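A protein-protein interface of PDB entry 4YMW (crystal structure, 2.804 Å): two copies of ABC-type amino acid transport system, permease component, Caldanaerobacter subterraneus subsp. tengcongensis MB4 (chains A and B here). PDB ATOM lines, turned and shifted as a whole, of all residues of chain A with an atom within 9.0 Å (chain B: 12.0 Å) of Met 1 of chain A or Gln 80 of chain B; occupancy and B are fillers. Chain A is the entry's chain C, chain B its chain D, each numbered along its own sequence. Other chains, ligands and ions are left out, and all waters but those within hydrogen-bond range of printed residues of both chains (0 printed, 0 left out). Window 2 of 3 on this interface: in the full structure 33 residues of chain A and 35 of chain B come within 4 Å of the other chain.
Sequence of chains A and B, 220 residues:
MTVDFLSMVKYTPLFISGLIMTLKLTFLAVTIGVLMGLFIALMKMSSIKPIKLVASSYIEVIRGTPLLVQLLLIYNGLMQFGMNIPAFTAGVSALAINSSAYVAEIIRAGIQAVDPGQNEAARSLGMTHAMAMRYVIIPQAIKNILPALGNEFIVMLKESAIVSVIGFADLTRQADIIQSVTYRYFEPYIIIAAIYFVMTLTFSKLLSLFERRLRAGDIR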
ATOM      1  N   MET A   1       7.532 -36.176  14.921  1.00  0.00           N
ATOM      2  CA  MET A   1       7.041 -37.241  15.791  1.00  0.00           C
ATOM      3  C   MET A   1       5.524 -37.103  16.019  1.00  0.00           C
ATOM      4  O   MET A   1       4.715 -37.561  15.200  1.00  0.00           O
ATOM      5  CB  MET A   1       7.779 -37.216  17.128  1.00  0.00           C
ATOM      6  CG  MET A   1       7.411 -38.357  18.072  1.00  0.00           C
ATOM      7  SD  MET A   1       8.363 -38.261  19.598  1.00  0.00           S
ATOM      8  CE  MET A   1       9.862 -37.453  19.021  1.00  0.00           C
ATOM      9  N   THR A   2       5.157 -36.514  17.163  1.00  0.00           N
ATOM     10  CA  THR A   2       3.786 -36.085  17.483  1.00  0.00           C
ATOM     11  C   THR A   2       3.862 -34.745  18.250  1.00  0.00           C
ATOM     12  O   THR A   2       4.962 -34.248  18.513  1.00  0.00           O
ATOM     13  CB  THR A   2       2.980 -37.143  18.299  1.00  0.00           C
ATOM     14  OG1 THR A   2       3.646 -37.443  19.534  1.00  0.00           O
ATOM     15  CG2 THR A   2       2.769 -38.412  17.490  1.00  0.00           C
ATOM     16  N   VAL A   3       2.703 -34.174  18.585  1.00  0.00           N
ATOM     17  CA  VAL A   3       2.578 -32.824  19.162  1.00  0.00           C
ATOM     18  C   VAL A   3       3.508 -32.524  20.354  1.00  0.00           C
ATOM     19  O   VAL A   3       3.601 -33.326  21.285  1.00  0.00           O
ATOM     20  CB  VAL A   3       1.115 -32.574  19.608  1.00  0.00           C
ATOM     21  CG1 VAL A   3       1.023 -31.382  20.555  1.00  0.00           C
ATOM     22  CG2 VAL A   3       0.218 -32.369  18.398  1.00  0.00           C
ATOM     23  N   ASP A   4       4.191 -31.373  20.308  1.00  0.00           N
ATOM     24  CA  ASP A   4       5.000 -30.874  21.430  1.00  0.00           C
ATOM     25  C   ASP A   4       5.221 -29.360  21.279  1.00  0.00           C
ATOM     26  O   ASP A   4       5.958 -28.914  20.400  1.00  0.00           O
ATOM     27  CB  ASP A   4       6.336 -31.663  21.492  1.00  0.00           C
ATOM     28  CG  ASP A   4       7.432 -31.013  22.382  1.00  0.00           C
ATOM     29  OD1 ASP A   4       7.395 -29.812  22.733  1.00  0.00           O
ATOM     30  OD2 ASP A   4       8.372 -31.753  22.748  1.00  0.00           O
ATOM     31  N   PHE A   5       4.601 -28.563  22.147  1.00  0.00           N
ATOM     32  CA  PHE A   5       4.724 -27.112  22.016  1.00  0.00           C
ATOM     33  C   PHE A   5       5.847 -26.477  22.862  1.00  0.00           C
ATOM     34  O   PHE A   5       6.347 -25.408  22.504  1.00  0.00           O
ATOM     35  CB  PHE A   5       3.376 -26.434  22.329  1.00  0.00           C
ATOM     36  CG  PHE A   5       2.386 -26.497  21.189  1.00  0.00           C
ATOM     37  CD1 PHE A   5       2.475 -25.613  20.126  1.00  0.00           C
ATOM     38  CD2 PHE A   5       1.377 -27.452  21.175  1.00  0.00           C
ATOM     39  CE1 PHE A   5       1.577 -25.681  19.068  1.00  0.00           C
ATOM     40  CE2 PHE A   5       0.476 -27.523  20.124  1.00  0.00           C
ATOM     41  CZ  PHE A   5       0.575 -26.638  19.070  1.00  0.00           C
ATOM     42  N   MET A   8       8.872 -25.453  21.284  1.00  0.00           N
ATOM     43  CA  MET A   8       8.781 -24.246  20.484  1.00  0.00           C
ATOM     44  C   MET A   8       9.216 -23.001  21.258  1.00  0.00           C
ATOM     45  O   MET A   8       9.673 -22.027  20.660  1.00  0.00           O
ATOM     46  CB  MET A   8       7.352 -24.078  19.979  1.00  0.00           C
ATOM     47  CG  MET A   8       7.248 -23.561  18.561  1.00  0.00           C
ATOM     48  SD  MET A   8       8.146 -24.611  17.416  1.00  0.00           S
ATOM     49  CE  MET A   8       7.307 -26.164  17.687  1.00  0.00           C
ATOM     50  N   ALA A 175       8.091 -20.599   9.939  1.00  0.00           N
ATOM     51  CA  ALA A 175       7.749 -22.012  10.010  1.00  0.00           C
ATOM     52  C   ALA A 175       8.726 -22.856   9.188  1.00  0.00           C
ATOM     53  O   ALA A 175       9.113 -23.955   9.601  1.00  0.00           O
ATOM     54  CB  ALA A 175       6.342 -22.237   9.545  1.00  0.00           C
ATOM     55  N   GLN A 179      11.241 -25.451  10.978  1.00  0.00           N
ATOM     56  CA  GLN A 179      11.117 -26.869  10.618  1.00  0.00           C
ATOM     57  C   GLN A 179      12.484 -27.401  10.152  1.00  0.00           C
ATOM     58  O   GLN A 179      12.817 -28.574  10.349  1.00  0.00           O
ATOM     59  CB  GLN A 179      10.052 -27.094   9.531  1.00  0.00           C
ATOM     60  CG  GLN A 179       9.959 -28.551   8.983  1.00  0.00           C
ATOM     61  CD  GLN A 179      10.967 -28.879   7.884  1.00  0.00           C
ATOM     62  OE1 GLN A 179      11.706 -28.008   7.415  1.00  0.00           O
ATOM     63  NE2 GLN A 179      11.016 -30.148   7.490  1.00  0.00           N
ATOM     64  N   THR A 182      13.790 -28.601  13.385  1.00  0.00           N
ATOM     65  CA  THR A 182      12.960 -29.396  14.302  1.00  0.00           C
ATOM     66  C   THR A 182      12.181 -30.487  13.578  1.00  0.00           C
ATOM     67  O   THR A 182      11.625 -31.390  14.210  1.00  0.00           O
ATOM     68  CB  THR A 182      11.954 -28.508  15.091  1.00  0.00           C
ATOM     69  OG1 THR A 182      11.025 -27.897  14.182  1.00  0.00           O
ATOM     70  CG2 THR A 182      12.690 -27.426  15.894  1.00  0.00           C
ATOM     71  N   TYR A 183      12.127 -30.368  12.253  1.00  0.00           N
ATOM     72  CA  TYR A 183      11.363 -31.267  11.386  1.00  0.00           C
ATOM     73  C   TYR A 183       9.860 -31.159  11.681  1.00  0.00           C
ATOM     74  O   TYR A 183       9.071 -32.034  11.316  1.00  0.00           O
ATOM     75  CB  TYR A 183      11.897 -32.706  11.534  1.00  0.00           C
ATOM     76  CG  TYR A 183      13.413 -32.737  11.393  1.00  0.00           C
ATOM     77  CD1 TYR A 183      14.014 -32.680  10.141  1.00  0.00           C
ATOM     78  CD2 TYR A 183      14.242 -32.754  12.516  1.00  0.00           C
ATOM     79  CE1 TYR A 183      15.395 -32.666  10.008  1.00  0.00           C
ATOM     80  CE2 TYR A 183      15.622 -32.736  12.393  1.00  0.00           C
ATOM     81  CZ  TYR A 183      16.193 -32.696  11.137  1.00  0.00           C
ATOM     82  OH  TYR A 183      17.566 -32.687  11.009  1.00  0.00           O
ATOM     83  N   ARG A 184       9.480 -30.056  12.327  1.00  0.00           N
ATOM     84  CA  ARG A 184       8.085 -29.793  12.714  1.00  0.00           C
ATOM     85  C   ARG A 184       7.452 -28.650  11.914  1.00  0.00           C
ATOM     86  O   ARG A 184       8.015 -27.557  11.819  1.00  0.00           O
ATOM     87  CB  ARG A 184       7.994 -29.478  14.212  1.00  0.00           C
ATOM     88  CG  ARG A 184       8.362 -30.643  15.112  1.00  0.00           C
ATOM     89  CD  ARG A 184       8.108 -30.344  16.582  1.00  0.00           C
ATOM     90  NE  ARG A 184       8.320 -31.511  17.437  1.00  0.00           N
ATOM     91  CZ  ARG A 184       7.507 -32.562  17.498  1.00  0.00           C
ATOM     92  NH1 ARG A 184       6.410 -32.605  16.756  1.00  0.00           N
ATOM     93  NH2 ARG A 184       7.787 -33.579  18.303  1.00  0.00           N
ATOM     94  N   TYR A 185       6.287 -28.916  11.334  1.00  0.00           N
ATOM     95  CA  TYR A 185       5.552 -27.901  10.587  1.00  0.00           C
ATOM     96  C   TYR A 185       4.275 -27.408  11.296  1.00  0.00           C
ATOM     97  O   TYR A 185       4.072 -26.205  11.430  1.00  0.00           O
ATOM     98  CB  TYR A 185       5.206 -28.440   9.202  1.00  0.00           C
ATOM     99  CG  TYR A 185       6.204 -28.084   8.123  1.00  0.00           C
ATOM    100  CD1 TYR A 185       6.671 -26.787   7.987  1.00  0.00           C
ATOM    101  CD2 TYR A 185       6.658 -29.040   7.221  1.00  0.00           C
ATOM    102  CE1 TYR A 185       7.560 -26.451   6.982  1.00  0.00           C
ATOM    103  CE2 TYR A 185       7.550 -28.716   6.214  1.00  0.00           C
ATOM    104  CZ  TYR A 185       8.000 -27.425   6.098  1.00  0.00           C
ATOM    105  OH  TYR A 185       8.893 -27.099   5.096  1.00  0.00           O
ATOM    106  N   PHE A 186       3.436 -28.345  11.741  1.00  0.00           N
ATOM    107  CA  PHE A 186       2.155 -28.073  12.409  1.00  0.00           C
ATOM    108  C   PHE A 186       2.223 -26.973  13.460  1.00  0.00           C
ATOM    109  O   PHE A 186       1.696 -25.872  13.280  1.00  0.00           O
ATOM    110  CB  PHE A 186       1.676 -29.364  13.061  1.00  0.00           C
ATOM    111  CG  PHE A 186       0.331 -29.284  13.707  1.00  0.00           C
ATOM    112  CD1 PHE A 186      -0.804 -29.690  13.019  1.00  0.00           C
ATOM    113  CD2 PHE A 186       0.203 -28.882  15.031  1.00  0.00           C
ATOM    114  CE1 PHE A 186      -2.052 -29.664  13.625  1.00  0.00           C
ATOM    115  CE2 PHE A 186      -1.044 -28.847  15.650  1.00  0.00           C
ATOM    116  CZ  PHE A 186      -2.175 -29.242  14.944  1.00  0.00           C
ATOM    117  N   GLU A 187       2.892 -27.303  14.553  1.00  0.00           N
ATOM    118  CA  GLU A 187       3.077 -26.442  15.714  1.00  0.00           C
ATOM    119  C   GLU A 187       3.581 -25.018  15.394  1.00  0.00           C
ATOM    120  O   GLU A 187       2.978 -24.038  15.837  1.00  0.00           O
ATOM    121  CB  GLU A 187       4.001 -27.185  16.671  1.00  0.00           C
ATOM    122  CG  GLU A 187       3.549 -28.652  16.722  1.00  0.00           C
ATOM    123  CD  GLU A 187       4.690 -29.653  16.736  1.00  0.00           C
ATOM    124  OE1 GLU A 187       5.376 -29.728  17.771  1.00  0.00           O
ATOM    125  OE2 GLU A 187       4.915 -30.335  15.704  1.00  0.00           O
ATOM    126  N   PRO A 188       4.687 -24.877  14.644  1.00  0.00           N
ATOM    127  CA  PRO A 188       5.058 -23.482  14.376  1.00  0.00           C
ATOM    128  C   PRO A 188       4.024 -22.747  13.508  1.00  0.00           C
ATOM    129  O   PRO A 188       3.945 -21.521  13.554  1.00  0.00           O
ATOM    130  CB  PRO A 188       6.403 -23.612  13.648  1.00  0.00           C
ATOM    131  CG  PRO A 188       6.372 -24.935  13.042  1.00  0.00           C
ATOM    132  CD  PRO A 188       5.622 -25.812  13.999  1.00  0.00           C
ATOM    133  N   TYR A 189       3.247 -23.483  12.723  1.00  0.00           N
ATOM    134  CA  TYR A 189       2.185 -22.851  11.962  1.00  0.00           C
ATOM    135  C   TYR A 189       1.054 -22.390  12.897  1.00  0.00           C
ATOM    136  O   TYR A 189       0.709 -21.219  12.873  1.00  0.00           O
ATOM    137  CB  TYR A 189       1.666 -23.785  10.865  1.00  0.00           C
ATOM    138  CG  TYR A 189       2.434 -23.599   9.585  1.00  0.00           C
ATOM    139  CD1 TYR A 189       2.760 -22.328   9.131  1.00  0.00           C
ATOM    140  CD2 TYR A 189       2.899 -24.684   8.865  1.00  0.00           C
ATOM    141  CE1 TYR A 189       3.488 -22.141   7.957  1.00  0.00           C
ATOM    142  CE2 TYR A 189       3.636 -24.513   7.708  1.00  0.00           C
ATOM    143  CZ  TYR A 189       3.933 -23.243   7.261  1.00  0.00           C
ATOM    144  OH  TYR A 189       4.669 -23.084   6.109  1.00  0.00           O
ATOM    145  N   VAL B  69      -1.283 -19.336   5.422  1.00  0.00           N
ATOM    146  CA  VAL B  69      -0.968 -20.153   6.592  1.00  0.00           C
ATOM    147  C   VAL B  69      -1.944 -21.307   6.732  1.00  0.00           C
ATOM    148  O   VAL B  69      -1.560 -22.375   7.147  1.00  0.00           O
ATOM    149  CB  VAL B  69      -0.950 -19.322   7.882  1.00  0.00           C
ATOM    150  CG1 VAL B  69      -0.608 -20.181   9.066  1.00  0.00           C
ATOM    151  CG2 VAL B  69       0.059 -18.178   7.756  1.00  0.00           C
ATOM    152  N   LEU B  71      -3.423 -22.919   4.226  1.00  0.00           N
ATOM    153  CA  LEU B  71      -3.054 -23.858   3.176  1.00  0.00           C
ATOM    154  C   LEU B  71      -1.867 -24.700   3.650  1.00  0.00           C
ATOM    155  O   LEU B  71      -1.937 -25.942   3.697  1.00  0.00           O
ATOM    156  CB  LEU B  71      -2.699 -23.111   1.881  1.00  0.00           C
ATOM    157  CG  LEU B  71      -2.287 -23.903   0.633  1.00  0.00           C
ATOM    158  CD1 LEU B  71      -3.497 -24.580   0.026  1.00  0.00           C
ATOM    159  CD2 LEU B  71      -1.614 -23.034  -0.401  1.00  0.00           C
ATOM    160  N   LEU B  72      -0.805 -24.009   4.065  1.00  0.00           N
ATOM    161  CA  LEU B  72       0.402 -24.669   4.562  1.00  0.00           C
ATOM    162  C   LEU B  72       0.137 -25.532   5.806  1.00  0.00           C
ATOM    163  O   LEU B  72       0.727 -26.591   5.940  1.00  0.00           O
ATOM    164  CB  LEU B  72       1.482 -23.626   4.865  1.00  0.00           C
ATOM    165  CG  LEU B  72       1.860 -22.766   3.649  1.00  0.00           C
ATOM    166  CD1 LEU B  72       3.038 -21.831   3.915  1.00  0.00           C
ATOM    167  CD2 LEU B  72       2.122 -23.627   2.412  1.00  0.00           C
ATOM    168  N   LEU B  73      -0.782 -25.131   6.680  1.00  0.00           N
ATOM    169  CA  LEU B  73      -1.071 -25.949   7.850  1.00  0.00           C
ATOM    170  C   LEU B  73      -1.799 -27.213   7.447  1.00  0.00           C
ATOM    171  O   LEU B  73      -1.668 -28.245   8.102  1.00  0.00           O
ATOM    172  CB  LEU B  73      -1.908 -25.193   8.880  1.00  0.00           C
ATOM    173  CG  LEU B  73      -2.203 -26.017  10.145  1.00  0.00           C
ATOM    174  CD1 LEU B  73      -1.028 -25.956  11.096  1.00  0.00           C
ATOM    175  CD2 LEU B  73      -3.491 -25.626  10.862  1.00  0.00           C
ATOM    176  N   ILE B  74      -2.567 -27.160   6.372  1.00  0.00           N
ATOM    177  CA  ILE B  74      -3.187 -28.402   5.924  1.00  0.00           C
ATOM    178  C   ILE B  74      -2.131 -29.300   5.257  1.00  0.00           C
ATOM    179  O   ILE B  74      -2.089 -30.509   5.500  1.00  0.00           O
ATOM    180  CB  ILE B  74      -4.375 -28.136   4.990  1.00  0.00           C
ATOM    181  CG1 ILE B  74      -5.494 -27.451   5.776  1.00  0.00           C
ATOM    182  CG2 ILE B  74      -4.916 -29.419   4.414  1.00  0.00           C
ATOM    183  CD1 ILE B  74      -6.766 -27.260   4.986  1.00  0.00           C
ATOM    184  N   TYR B  75      -1.264 -28.690   4.447  1.00  0.00           N
ATOM    185  CA  TYR B  75      -0.246 -29.398   3.644  1.00  0.00           C
ATOM    186  C   TYR B  75       0.980 -29.889   4.441  1.00  0.00           C
ATOM    187  O   TYR B  75       1.146 -31.080   4.703  1.00  0.00           O
ATOM    188  CB  TYR B  75       0.225 -28.464   2.529  1.00  0.00           C
ATOM    189  CG  TYR B  75       0.938 -29.108   1.362  1.00  0.00           C
ATOM    190  CD1 TYR B  75       2.285 -28.860   1.130  1.00  0.00           C
ATOM    191  CD2 TYR B  75       0.258 -29.925   0.463  1.00  0.00           C
ATOM    192  CE1 TYR B  75       2.946 -29.412   0.051  1.00  0.00           C
ATOM    193  CE2 TYR B  75       0.912 -30.482  -0.629  1.00  0.00           C
ATOM    194  CZ  TYR B  75       2.261 -30.221  -0.824  1.00  0.00           C
ATOM    195  OH  TYR B  75       2.925 -30.775  -1.894  1.00  0.00           O
ATOM    196  N   ASN B  76       1.816 -28.941   4.836  1.00  0.00           N
ATOM    197  CA  ASN B  76       3.026 -29.226   5.581  1.00  0.00           C
ATOM    198  C   ASN B  76       2.770 -29.686   7.006  1.00  0.00           C
ATOM    199  O   ASN B  76       3.403 -30.616   7.487  1.00  0.00           O
ATOM    200  CB  ASN B  76       3.922 -27.994   5.597  1.00  0.00           C
ATOM    201  CG  ASN B  76       4.402 -27.613   4.215  1.00  0.00           C
ATOM    202  OD1 ASN B  76       4.246 -28.379   3.267  1.00  0.00           O
ATOM    203  ND2 ASN B  76       5.005 -26.433   4.094  1.00  0.00           N
ATOM    204  N   GLY B  77       1.849 -29.034   7.691  1.00  0.00           N
ATOM    205  CA  GLY B  77       1.588 -29.367   9.075  1.00  0.00           C
ATOM    206  C   GLY B  77       1.066 -30.774   9.307  1.00  0.00           C
ATOM    207  O   GLY B  77       1.064 -31.241  10.442  1.00  0.00           O
ATOM    208  N   LEU B  78       0.660 -31.480   8.256  1.00  0.00           N
ATOM    209  CA  LEU B  78       0.060 -32.792   8.487  1.00  0.00           C
ATOM    210  C   LEU B  78       0.914 -33.979   8.038  1.00  0.00           C
ATOM    211  O   LEU B  78       0.515 -35.138   8.213  1.00  0.00           O
ATOM    212  CB  LEU B  78      -1.297 -32.866   7.787  1.00  0.00           C
ATOM    213  CG  LEU B  78      -2.473 -32.194   8.489  1.00  0.00           C
ATOM    214  CD1 LEU B  78      -3.771 -32.745   7.935  1.00  0.00           C
ATOM    215  CD2 LEU B  78      -2.386 -32.400   9.995  1.00  0.00           C
ATOM    216  N   MET B  79       2.103 -33.687   7.515  1.00  0.00           N
ATOM    217  CA  MET B  79       3.090 -34.708   7.171  1.00  0.00           C
ATOM    218  C   MET B  79       3.528 -35.473   8.400  1.00  0.00           C
ATOM    219  O   MET B  79       3.470 -36.707   8.439  1.00  0.00           O
ATOM    220  CB  MET B  79       4.291 -34.060   6.489  1.00  0.00           C
ATOM    221  CG  MET B  79       3.993 -33.626   5.074  1.00  0.00           C
ATOM    222  SD  MET B  79       5.393 -32.787   4.319  1.00  0.00           S
ATOM    223  CE  MET B  79       4.657 -32.067   2.844  1.00  0.00           C
ATOM    224  N   GLN B  80       3.937 -34.734   9.422  1.00  0.00           N
ATOM    225  CA  GLN B  80       4.497 -35.348  10.619  1.00  0.00           C
ATOM    226  C   GLN B  80       3.564 -36.292  11.370  1.00  0.00           C
ATOM    227  O   GLN B  80       3.981 -36.944  12.333  1.00  0.00           O
ATOM    228  CB  GLN B  80       4.970 -34.255  11.562  1.00  0.00           C
ATOM    229  CG  GLN B  80       3.891 -33.292  11.986  1.00  0.00           C
ATOM    230  CD  GLN B  80       4.476 -32.045  12.624  1.00  0.00           C
ATOM    231  OE1 GLN B  80       4.975 -31.150  11.928  1.00  0.00           O
ATOM    232  NE2 GLN B  80       4.428 -31.983  13.952  1.00  0.00           N
ATOM    233  N   PHE B  81       2.318 -36.392  10.918  1.00  0.00           N
ATOM    234  CA  PHE B  81       1.392 -37.358  11.494  1.00  0.00           C
ATOM    235  C   PHE B  81       1.257 -38.534  10.550  1.00  0.00           C
ATOM    236  O   PHE B  81       0.361 -39.374  10.683  1.00  0.00           O
ATOM    237  CB  PHE B  81       0.027 -36.725  11.772  1.00  0.00           C
ATOM    238  CG  PHE B  81       0.087 -35.521  12.669  1.00  0.00           C
ATOM    239  CD1 PHE B  81       0.507 -35.645  13.987  1.00  0.00           C
ATOM    240  CD2 PHE B  81      -0.289 -34.268  12.203  1.00  0.00           C
ATOM    241  CE1 PHE B  81       0.566 -34.535  14.824  1.00  0.00           C
ATOM    242  CE2 PHE B  81      -0.237 -33.151  13.035  1.00  0.00           C
ATOM    243  CZ  PHE B  81       0.192 -33.287  14.348  1.00  0.00           C
ATOM    244  N   GLY B  82       2.200 -38.597   9.616  1.00  0.00           N
ATOM    245  CA  GLY B  82       2.285 -39.680   8.656  1.00  0.00           C
ATOM    246  C   GLY B  82       1.117 -39.639   7.694  1.00  0.00           C
ATOM    247  O   GLY B  82       0.654 -40.670   7.205  1.00  0.00           O
ATOM    248  N   MET B  83       0.643 -38.432   7.425  1.00  0.00           N
ATOM    249  CA  MET B  83      -0.403 -38.208   6.446  1.00  0.00           C
ATOM    250  C   MET B  83       0.171 -37.273   5.398  1.00  0.00           C
ATOM    251  O   MET B  83       0.660 -36.198   5.728  1.00  0.00           O
ATOM    252  CB  MET B  83      -1.665 -37.602   7.087  1.00  0.00           C
ATOM    253  CG  MET B  83      -2.146 -38.155   8.448  1.00  0.00           C
ATOM    254  SD  MET B  83      -2.131 -39.962   8.662  1.00  0.00           S
ATOM    255  CE  MET B  83      -2.723 -40.111  10.340  1.00  0.00           C
ATOM    256  N   ASN B  84       0.138 -37.682   4.137  1.00  0.00           N
ATOM    257  CA  ASN B  84       0.518 -36.773   3.063  1.00  0.00           C
ATOM    258  C   ASN B  84      -0.565 -36.694   2.011  1.00  0.00           C
ATOM    259  O   ASN B  84      -0.682 -37.546   1.131  1.00  0.00           O
ATOM    260  CB  ASN B  84       1.844 -37.173   2.413  1.00  0.00           C
ATOM    261  CG  ASN B  84       2.179 -36.305   1.195  1.00  0.00           C
ATOM    262  OD1 ASN B  84       1.834 -36.645   0.058  1.00  0.00           O
ATOM    263  ND2 ASN B  84       2.822 -35.159   1.439  1.00  0.00           N
ATOM    264  N   ILE B  85      -1.368 -35.650   2.141  1.00  0.00           N
ATOM    265  CA  ILE B  85      -2.428 -35.338   1.206  1.00  0.00           C
ATOM    266  C   ILE B  85      -1.882 -34.680  -0.055  1.00  0.00           C
ATOM    267  O   ILE B  85      -0.955 -33.870   0.016  1.00  0.00           O
ATOM    268  CB  ILE B  85      -3.454 -34.413   1.876  1.00  0.00           C
ATOM    269  CG1 ILE B  85      -2.708 -33.256   2.531  1.00  0.00           C
ATOM    270  CG2 ILE B  85      -4.260 -35.169   2.943  1.00  0.00           C
ATOM    271  CD1 ILE B  85      -3.580 -32.275   3.156  1.00  0.00           C
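O of Asn 76 of chain B touches CB of Tyr 185 of chain A, 3.3 Å away. Tyr 185 of chain A touches Gly 77 of chain B. CD1 of Leu 73 of chain B touches O of Phe 186 of chain A, 3.5 Å away. CB of Phe 186 of chain A touches O of Gly 77 of chain B (3.3 Å). CE2 of Phe 81 of chain B touches CD1 of Phe 186 of chain A (3.5 Å). Val 69 of chain B touches Tyr 189 of chain A (CG1 to CD1, 3.99 Å). OH of Tyr 189 of chain A touches CD1 of Leu 72 of chain B, 3.0 Å away. Leu 73 of chain B touches Tyr 189 of chain A. Asn 76 of chain B touches Tyr 189 of chain A (ND2 to OH, 3.9 Å).
No position is printed for both chains.
The side-chain carboxylate (OE2) of Glu 187 of chain A is in hydrogen-bond range of the side-chain amide nitrogen (NE2) of Gln 80 of chain B, at 2.5 Å. The side-chain amide nitrogen (NE2) of Gln 80 of chain B lies close to the guanidinium group (NH1) of Arg 184 of chain A (3.5 Å). The side-chain amide oxygen (OE1) of Gln 80 of chain B is in hydrogen-bond range of the backbone NH (N) of Phe 186 of chain A, 3.2 Å away. O of Gln 80 of chain B lies close to O of Met 1 of chain A (3.0 Å). The backbone NH of Tyr 185 of chain A lies within hydrogen-bond range of the side-chain amide oxygen of Gln 80 of chain B (2.7 Å).
No residue of chain B comes within 4 Å of Thr 2 of chain A. No residue of chain B comes within 4 Å of Val 3 of chain A. Arg 184 of chain A touches just one residue of chain B: Gln 80. Phe 186 of chain A touches four residues of chain B. Pro 188 of chain A touches none of the printed residues of chain B. Of the printed residues of chain B, Tyr 189 of chain A touches Val 69, Leu 72, Leu 73 and Asn 76. Of the printed residues of chain A, Val 69 of chain B touches Tyr 189. Of the printed residues of chain A, Leu 72 of chain B touches Tyr 189. Of the printed residues of chain A, Leu 73 of chain B touches Phe 186 (3.5 Å) and Tyr 189 (3.5 Å). Of the printed residues of chain A, Asn 76 of chain B touches Tyr 185 (3.3 Å) and Tyr 189 (3.9 Å). Printed residues of chain A within 4 Å of Gln 80 of chain B: Met 1 (3.0 Å), Arg 184 (3.5 Å), Tyr 185 (2.7 Å), Phe 186 (3.2 Å) and Glu 187 (2.5 Å). The nearest printed residue of chain A that does not touch Asn 76 of chain B is Phe 186 of chain A (4.8 Å).
Printed residues of chain A that touch a printed residue of chain B: Met 1, Arg 184, Tyr 185, Phe 186, Glu 187 and Tyr 189. Hydrophobic or aromatic side chains of chain A that line the printed part of chain B: Tyr 185, Phe 186 and Tyr 189. Among the printed residues, 14 pairs touch across the chains.
The side-chain carboxylate of Glu 187 of chain A is in salt-bridge range of the guanidinium group of Arg 184 of chain A (2.9 Å). The backbone carbonyl oxygen (O) of Thr 2 of chain A is in hydrogen-bond range of the guanidinium group (NH1) of Arg 184 of chain A, 2.8 Å away. The backbone NH (N) of Asp 4 of chain A sits at hydrogen-bond distance from the side-chain carboxylate (OE1) of Glu 187 of chain A (3.2 Å). The backbone NH of Gly 77 of chain B lies within hydrogen-bond range of the backbone carbonyl oxygen of Leu 72 of chain B, 3.2 Å away. The side-chain hydroxyl of Thr 182 of chain A sits close to the backbone NH of Arg 184 of chain A, at 3.2 Å.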
